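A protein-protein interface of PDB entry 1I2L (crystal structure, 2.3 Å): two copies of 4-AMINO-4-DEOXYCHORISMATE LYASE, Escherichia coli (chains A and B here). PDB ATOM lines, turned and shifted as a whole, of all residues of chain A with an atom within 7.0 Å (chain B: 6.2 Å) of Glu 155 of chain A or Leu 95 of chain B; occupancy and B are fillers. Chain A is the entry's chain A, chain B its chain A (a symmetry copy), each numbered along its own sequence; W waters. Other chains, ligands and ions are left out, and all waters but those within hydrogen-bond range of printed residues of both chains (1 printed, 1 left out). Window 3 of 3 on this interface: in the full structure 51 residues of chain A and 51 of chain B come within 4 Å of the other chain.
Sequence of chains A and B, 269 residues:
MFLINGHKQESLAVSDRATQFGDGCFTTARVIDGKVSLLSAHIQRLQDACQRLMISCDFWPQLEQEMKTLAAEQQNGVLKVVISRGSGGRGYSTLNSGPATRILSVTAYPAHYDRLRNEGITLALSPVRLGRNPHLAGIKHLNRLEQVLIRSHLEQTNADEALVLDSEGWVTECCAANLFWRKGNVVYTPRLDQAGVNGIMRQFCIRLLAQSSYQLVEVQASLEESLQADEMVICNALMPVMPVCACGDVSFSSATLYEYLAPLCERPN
The side-chain carboxylate of Glu 155 of chain A lies within hydrogen-bond range of the side-chain hydroxyl of Ser 93 of chain B.
The guanidinium group (NH2) of Arg 151 of chain A sits close to the guanidinium group (NH2) of Arg 90 of chain B.
The backbone carbonyl oxygen of Ser 93 of chain B lies within hydrogen-bond range of the guanidinium group of Arg 17 of chain B.
N of Leu 95 of chain B is in hydrogen-bond range of OG of Ser 93 of chain B, at 3.1 Å.
O of Ser 152 of chain A lies close to NE2 of Gln 156 of chain A, at 3.3 Å.
The guanidinium group (NE) of Arg 151 of chain A lies within salt-bridge range of the side-chain carboxylate (OE2) of Glu 155 of chain A.
The guanidinium group (NH2) of Arg 17 of chain B lies within hydrogen-bond range of the backbone carbonyl oxygen (O) of Tyr 92 of chain B, 3.0 Å away.
O of Gly 88 of chain B is in hydrogen-bond range of NH1 of Arg 17 of chain B, at 3.2 Å.
Among the printed residues, pairs that only touch across the chains: Glu 155 of chain A with Leu 95 of chain B (3.3 Å), Val 148 of chain A with Thr 94 of chain B (3.5 Å), Val 148 of chain A with Arg 17 of chain B (3.5 Å), Val 148 of chain A with Tyr 92 of chain B (3.6 Å), Arg 151 of chain A with Ser 93 of chain B (3.7 Å), Ser 152 of chain A with Thr 94 of chain B (3.8 Å) and Ser 152 of chain A with Met 54 of chain B (3.8 Å).
Of the printed residues of chain B, Val 148 of chain A touches Arg 17, Tyr 92 and Thr 94.
Of the printed residues of chain A, Ser 93 of chain B touches Arg 151 and Glu 155.
Of the printed residues of chain A, Tyr 92 of chain B touches Val 148 (3.6 Å).
Ser 97 of chain B touches none of the printed residues of chain A.
The nearest residue of chain A that does not touch Leu 95 of chain B is Gln 156 of chain A (6.5 Å).
Hydrophobic or aromatic side chains of chain A that line the printed part of chain B: Val 148.
Of the 11 printed residues of chain B, 7 touch a printed residue of chain A.
Printed residues of chain B that touch a printed residue of chain A: Arg 17, Met 54, Arg 90, Tyr 92, Ser 93, Thr 94 and Leu 95.
Hydrophobic or aromatic side chains of chain B within 4 Å of the printed part of chain A: Met 54 and Leu 95.
No position is printed for both chains.
Of the 9 pairs that touch across the chains among the printed residues, none has its exchanged pair printed and touching as well.
Water W1 lies within hydrogen-bond range of OE2 of Glu 155 of chain A, NH2 of Arg 151 of chain A and NH2 of Arg 90 of chain B.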
ATOM      1  N   VAL A 148     -19.552  -6.054  -4.956  1.00  0.00           N
ATOM      2  CA  VAL A 148     -20.988  -5.840  -4.922  1.00  0.00           C
ATOM      3  C   VAL A 148     -21.672  -7.191  -4.660  1.00  0.00           C
ATOM      4  O   VAL A 148     -22.644  -7.283  -3.912  1.00  0.00           O
ATOM      5  CB  VAL A 148     -21.496  -5.231  -6.245  1.00  0.00           C
ATOM      6  CG1 VAL A 148     -23.020  -5.123  -6.237  1.00  0.00           C
ATOM      7  CG2 VAL A 148     -20.871  -3.858  -6.454  1.00  0.00           C
ATOM      8  N   ILE A 150     -20.259  -9.804  -3.161  1.00  0.00           N
ATOM      9  CA  ILE A 150     -19.938 -10.227  -1.807  1.00  0.00           C
ATOM     10  C   ILE A 150     -20.889  -9.516  -0.848  1.00  0.00           C
ATOM     11  O   ILE A 150     -21.450 -10.137   0.043  1.00  0.00           O
ATOM     12  CB  ILE A 150     -18.468  -9.880  -1.442  1.00  0.00           C
ATOM     13  CG1 ILE A 150     -17.511 -10.711  -2.303  1.00  0.00           C
ATOM     14  CG2 ILE A 150     -18.249 -10.080   0.056  1.00  0.00           C
ATOM     15  CD1 ILE A 150     -16.046 -10.229  -2.301  1.00  0.00           C
ATOM     16  N   ARG A 151     -21.068  -8.215  -1.045  1.00  0.00           N
ATOM     17  CA  ARG A 151     -21.941  -7.430  -0.187  1.00  0.00           C
ATOM     18  C   ARG A 151     -23.388  -7.910  -0.192  1.00  0.00           C
ATOM     19  O   ARG A 151     -24.027  -7.968   0.866  1.00  0.00           O
ATOM     20  CB  ARG A 151     -21.911  -5.955  -0.582  1.00  0.00           C
ATOM     21  CG  ARG A 151     -22.656  -5.048   0.394  1.00  0.00           C
ATOM     22  CD  ARG A 151     -21.845  -4.845   1.656  1.00  0.00           C
ATOM     23  NE  ARG A 151     -22.687  -4.658   2.833  1.00  0.00           N
ATOM     24  CZ  ARG A 151     -22.216  -4.511   4.075  1.00  0.00           C
ATOM     25  NH1 ARG A 151     -20.902  -4.518   4.296  1.00  0.00           N
ATOM     26  NH2 ARG A 151     -23.056  -4.392   5.105  1.00  0.00           N
ATOM     27  N   SER A 152     -23.908  -8.240  -1.370  1.00  0.00           N
ATOM     28  CA  SER A 152     -25.286  -8.707  -1.468  1.00  0.00           C
ATOM     29  C   SER A 152     -25.487  -9.984  -0.667  1.00  0.00           C
ATOM     30  O   SER A 152     -26.516 -10.146  -0.007  1.00  0.00           O
ATOM     31  CB  SER A 152     -25.666  -8.974  -2.916  1.00  0.00           C
ATOM     32  OG  SER A 152     -25.166  -7.952  -3.731  1.00  0.00           O
ATOM     33  N   HIS A 153     -24.519 -10.896  -0.734  1.00  0.00           N
ATOM     34  CA  HIS A 153     -24.632 -12.132   0.025  1.00  0.00           C
ATOM     35  C   HIS A 153     -24.532 -11.860   1.524  1.00  0.00           C
ATOM     36  O   HIS A 153     -25.254 -12.460   2.319  1.00  0.00           O
ATOM     37  CB  HIS A 153     -23.562 -13.121  -0.424  1.00  0.00           C
ATOM     38  CG  HIS A 153     -23.835 -13.720  -1.770  1.00  0.00           C
ATOM     39  ND1 HIS A 153     -24.431 -14.952  -1.927  1.00  0.00           N
ATOM     40  CD2 HIS A 153     -23.668 -13.220  -3.020  1.00  0.00           C
ATOM     41  CE1 HIS A 153     -24.625 -15.184  -3.214  1.00  0.00           C
ATOM     42  NE2 HIS A 153     -24.173 -14.148  -3.897  1.00  0.00           N
ATOM     43  N   LEU A 154     -23.649 -10.934   1.888  1.00  0.00           N
ATOM     44  CA  LEU A 154     -23.417 -10.543   3.271  1.00  0.00           C
ATOM     45  C   LEU A 154     -24.693 -10.024   3.922  1.00  0.00           C
ATOM     46  O   LEU A 154     -24.930 -10.249   5.103  1.00  0.00           O
ATOM     47  CB  LEU A 154     -22.328  -9.456   3.348  1.00  0.00           C
ATOM     48  CG  LEU A 154     -22.127  -8.771   4.705  1.00  0.00           C
ATOM     49  CD1 LEU A 154     -21.745  -9.820   5.768  1.00  0.00           C
ATOM     50  CD2 LEU A 154     -21.032  -7.713   4.586  1.00  0.00           C
ATOM     51  N   GLU A 155     -25.515  -9.330   3.149  1.00  0.00           N
ATOM     52  CA  GLU A 155     -26.757  -8.786   3.679  1.00  0.00           C
ATOM     53  C   GLU A 155     -27.787  -9.875   3.969  1.00  0.00           C
ATOM     54  O   GLU A 155     -28.762  -9.638   4.690  1.00  0.00           O
ATOM     55  CB  GLU A 155     -27.299  -7.729   2.712  1.00  0.00           C
ATOM     56  CG  GLU A 155     -26.409  -6.483   2.702  1.00  0.00           C
ATOM     57  CD  GLU A 155     -26.660  -5.584   1.513  1.00  0.00           C
ATOM     58  OE1 GLU A 155     -27.052  -6.110   0.455  1.00  0.00           O
ATOM     59  OE2 GLU A 155     -26.446  -4.361   1.625  1.00  0.00           O
ATOM     60  N   GLN A 156     -27.539 -11.069   3.429  1.00  0.00           N
ATOM     61  CA  GLN A 156     -28.421 -12.218   3.628  1.00  0.00           C
ATOM     62  C   GLN A 156     -28.095 -12.894   4.962  1.00  0.00           C
ATOM     63  O   GLN A 156     -28.689 -13.912   5.311  1.00  0.00           O
ATOM     64  CB  GLN A 156     -28.238 -13.245   2.513  1.00  0.00           C
ATOM     65  CG  GLN A 156     -28.218 -12.670   1.133  1.00  0.00           C
ATOM     66  CD  GLN A 156     -29.566 -12.202   0.679  1.00  0.00           C
ATOM     67  OE1 GLN A 156     -30.513 -12.982   0.604  1.00  0.00           O
ATOM     68  NE2 GLN A 156     -29.668 -10.918   0.360  1.00  0.00           N
ATOM     69  N   THR A 157     -27.138 -12.325   5.693  1.00  0.00           N
ATOM     70  CA  THR A 157     -26.727 -12.851   6.989  1.00  0.00           C
ATOM     71  C   THR A 157     -26.810 -11.718   8.020  1.00  0.00           C
ATOM     72  O   THR A 157     -27.159 -10.579   7.681  1.00  0.00           O
ATOM     73  CB  THR A 157     -25.269 -13.371   6.948  1.00  0.00           C
ATOM     74  OG1 THR A 157     -24.367 -12.256   6.862  1.00  0.00           O
ATOM     75  CG2 THR A 157     -25.051 -14.295   5.752  1.00  0.00           C
ATOM     76  N   ASN A 158     -26.473 -12.026   9.272  1.00  0.00           N
ATOM     77  CA  ASN A 158     -26.512 -11.034  10.352  1.00  0.00           C
ATOM     78  C   ASN A 158     -25.117 -10.461  10.643  1.00  0.00           C
ATOM     79  O   ASN A 158     -24.918  -9.769  11.647  1.00  0.00           O
ATOM     80  CB  ASN A 158     -27.070 -11.682  11.630  1.00  0.00           C
ATOM     81  CG  ASN A 158     -27.502 -10.661  12.681  1.00  0.00           C
ATOM     82  OD1 ASN A 158     -27.512 -10.968  13.874  1.00  0.00           O
ATOM     83  ND2 ASN A 158     -27.878  -9.456  12.245  1.00  0.00           N
ATOM     84  N   ALA A 159     -24.154 -10.749   9.771  1.00  0.00           N
ATOM     85  CA  ALA A 159     -22.790 -10.272   9.965  1.00  0.00           C
ATOM     86  C   ALA A 159     -22.599  -8.871   9.420  1.00  0.00           C
ATOM     87  O   ALA A 159     -23.290  -8.453   8.495  1.00  0.00           O
ATOM     88  CB  ALA A 159     -21.807 -11.223   9.312  1.00  0.00           C
ATOM     89  N   ARG B  17     -23.651   3.522 -10.846  1.00  0.00           N
ATOM     90  CA  ARG B  17     -22.766   2.447 -10.474  1.00  0.00           C
ATOM     91  C   ARG B  17     -21.933   1.850 -11.605  1.00  0.00           C
ATOM     92  O   ARG B  17     -20.913   1.204 -11.350  1.00  0.00           O
ATOM     93  CB  ARG B  17     -23.571   1.403  -9.703  1.00  0.00           C
ATOM     94  CG  ARG B  17     -24.058   1.988  -8.356  1.00  0.00           C
ATOM     95  CD  ARG B  17     -25.153   1.173  -7.761  1.00  0.00           C
ATOM     96  NE  ARG B  17     -24.678  -0.159  -7.415  1.00  0.00           N
ATOM     97  CZ  ARG B  17     -24.333  -0.531  -6.189  1.00  0.00           C
ATOM     98  NH1 ARG B  17     -24.422   0.339  -5.185  1.00  0.00           N
ATOM     99  NH2 ARG B  17     -23.879  -1.764  -5.972  1.00  0.00           N
ATOM    100  N   MET B  54     -28.475  -9.605 -10.239  1.00  0.00           N
ATOM    101  CA  MET B  54     -29.536  -9.194  -9.342  1.00  0.00           C
ATOM    102  C   MET B  54     -30.054  -7.797  -9.686  1.00  0.00           C
ATOM    103  O   MET B  54     -30.515  -7.059  -8.822  1.00  0.00           O
ATOM    104  CB  MET B  54     -29.039  -9.250  -7.890  1.00  0.00           C
ATOM    105  CG  MET B  54     -30.131  -9.069  -6.867  1.00  0.00           C
ATOM    106  SD  MET B  54     -29.593  -9.245  -5.136  1.00  0.00           S
ATOM    107  CE  MET B  54     -28.825  -7.607  -4.846  1.00  0.00           C
ATOM    108  N   GLY B  88     -27.284   4.923  -6.287  1.00  0.00           N
ATOM    109  CA  GLY B  88     -27.761   4.517  -4.977  1.00  0.00           C
ATOM    110  C   GLY B  88     -26.910   3.524  -4.216  1.00  0.00           C
ATOM    111  O   GLY B  88     -25.799   3.163  -4.639  1.00  0.00           O
ATOM    112  N   GLY B  89     -27.453   3.087  -3.083  1.00  0.00           N
ATOM    113  CA  GLY B  89     -26.776   2.131  -2.235  1.00  0.00           C
ATOM    114  C   GLY B  89     -25.624   2.774  -1.491  1.00  0.00           C
ATOM    115  O   GLY B  89     -25.004   3.732  -1.981  1.00  0.00           O
ATOM    116  N   ARG B  90     -25.348   2.267  -0.293  1.00  0.00           N
ATOM    117  CA  ARG B  90     -24.239   2.783   0.497  1.00  0.00           C
ATOM    118  C   ARG B  90     -23.052   1.865   0.204  1.00  0.00           C
ATOM    119  O   ARG B  90     -23.136   0.652   0.399  1.00  0.00           O
ATOM    120  CB  ARG B  90     -24.584   2.790   1.998  1.00  0.00           C
ATOM    121  CG  ARG B  90     -24.588   1.431   2.730  1.00  0.00           C
ATOM    122  CD  ARG B  90     -24.765   1.666   4.248  1.00  0.00           C
ATOM    123  NE  ARG B  90     -24.972   0.451   5.042  1.00  0.00           N
ATOM    124  CZ  ARG B  90     -24.035  -0.461   5.292  1.00  0.00           C
ATOM    125  NH1 ARG B  90     -22.803  -0.312   4.809  1.00  0.00           N
ATOM    126  NH2 ARG B  90     -24.326  -1.520   6.039  1.00  0.00           N
ATOM    127  N   TYR B  92     -20.718  -0.609  -1.591  1.00  0.00           N
ATOM    128  CA  TYR B  92     -21.006  -1.633  -2.591  1.00  0.00           C
ATOM    129  C   TYR B  92     -22.434  -2.181  -2.516  1.00  0.00           C
ATOM    130  O   TYR B  92     -22.885  -2.880  -3.424  1.00  0.00           O
ATOM    131  CB  TYR B  92     -20.017  -2.796  -2.459  1.00  0.00           C
ATOM    132  CG  TYR B  92     -18.562  -2.394  -2.614  1.00  0.00           C
ATOM    133  CD1 TYR B  92     -18.092  -1.862  -3.808  1.00  0.00           C
ATOM    134  CD2 TYR B  92     -17.657  -2.552  -1.561  1.00  0.00           C
ATOM    135  CE1 TYR B  92     -16.765  -1.502  -3.952  1.00  0.00           C
ATOM    136  CE2 TYR B  92     -16.326  -2.196  -1.694  1.00  0.00           C
ATOM    137  CZ  TYR B  92     -15.889  -1.674  -2.895  1.00  0.00           C
ATOM    138  OH  TYR B  92     -14.571  -1.360  -3.066  1.00  0.00           O
ATOM    139  N   SER B  93     -23.148  -1.853  -1.447  1.00  0.00           N
ATOM    140  CA  SER B  93     -24.512  -2.343  -1.269  1.00  0.00           C
ATOM    141  C   SER B  93     -25.470  -1.992  -2.392  1.00  0.00           C
ATOM    142  O   SER B  93     -25.454  -0.881  -2.907  1.00  0.00           O
ATOM    143  CB  SER B  93     -25.091  -1.825   0.048  1.00  0.00           C
ATOM    144  OG  SER B  93     -26.410  -2.300   0.239  1.00  0.00           O
ATOM    145  N   THR B  94     -26.309  -2.954  -2.757  1.00  0.00           N
ATOM    146  CA  THR B  94     -27.318  -2.768  -3.794  1.00  0.00           C
ATOM    147  C   THR B  94     -28.651  -2.311  -3.154  1.00  0.00           C
ATOM    148  O   THR B  94     -29.593  -1.920  -3.851  1.00  0.00           O
ATOM    149  CB  THR B  94     -27.571  -4.086  -4.553  1.00  0.00           C
ATOM    150  OG1 THR B  94     -28.103  -5.069  -3.648  1.00  0.00           O
ATOM    151  CG2 THR B  94     -26.266  -4.611  -5.152  1.00  0.00           C
ATOM    152  N   LEU B  95     -28.720  -2.358  -1.824  1.00  0.00           N
ATOM    153  CA  LEU B  95     -29.926  -1.953  -1.114  1.00  0.00           C
ATOM    154  C   LEU B  95     -30.259  -0.486  -1.350  1.00  0.00           C
ATOM    155  O   LEU B  95     -29.408   0.382  -1.214  1.00  0.00           O
ATOM    156  CB  LEU B  95     -29.779  -2.225   0.388  1.00  0.00           C
ATOM    157  CG  LEU B  95     -29.584  -3.710   0.712  1.00  0.00           C
ATOM    158  CD1 LEU B  95     -29.647  -3.942   2.214  1.00  0.00           C
ATOM    159  CD2 LEU B  95     -30.663  -4.521  -0.007  1.00  0.00           C
ATOM    160  N   ASN B  96     -31.509  -0.233  -1.721  1.00  0.00           N
ATOM    161  CA  ASN B  96     -31.991   1.118  -1.993  1.00  0.00           C
ATOM    162  C   ASN B  96     -31.425   1.710  -3.283  1.00  0.00           C
ATOM    163  O   ASN B  96     -31.545   2.909  -3.518  1.00  0.00           O
ATOM    164  CB  ASN B  96     -31.677   2.048  -0.808  1.00  0.00           C
ATOM    165  CG  ASN B  96     -32.237   1.518   0.506  1.00  0.00           C
ATOM    166  OD1 ASN B  96     -33.348   0.978   0.543  1.00  0.00           O
ATOM    167  ND2 ASN B  96     -31.472   1.667   1.587  1.00  0.00           N
ATOM    168  N   SER B  97     -30.812   0.870  -4.113  1.00  0.00           N
ATOM    169  CA  SER B  97     -30.254   1.334  -5.380  1.00  0.00           C
ATOM    170  C   SER B  97     -31.310   1.214  -6.478  1.00  0.00           C
ATOM    171  O   SER B  97     -32.314   0.531  -6.313  1.00  0.00           O
ATOM    172  CB  SER B  97     -29.054   0.487  -5.779  1.00  0.00           C
ATOM    173  OG  SER B  97     -29.509  -0.762  -6.272  1.00  0.00           O
HETATM  174  O   HOH W   1     -25.723  -3.307   3.711  1.00  0.00           O
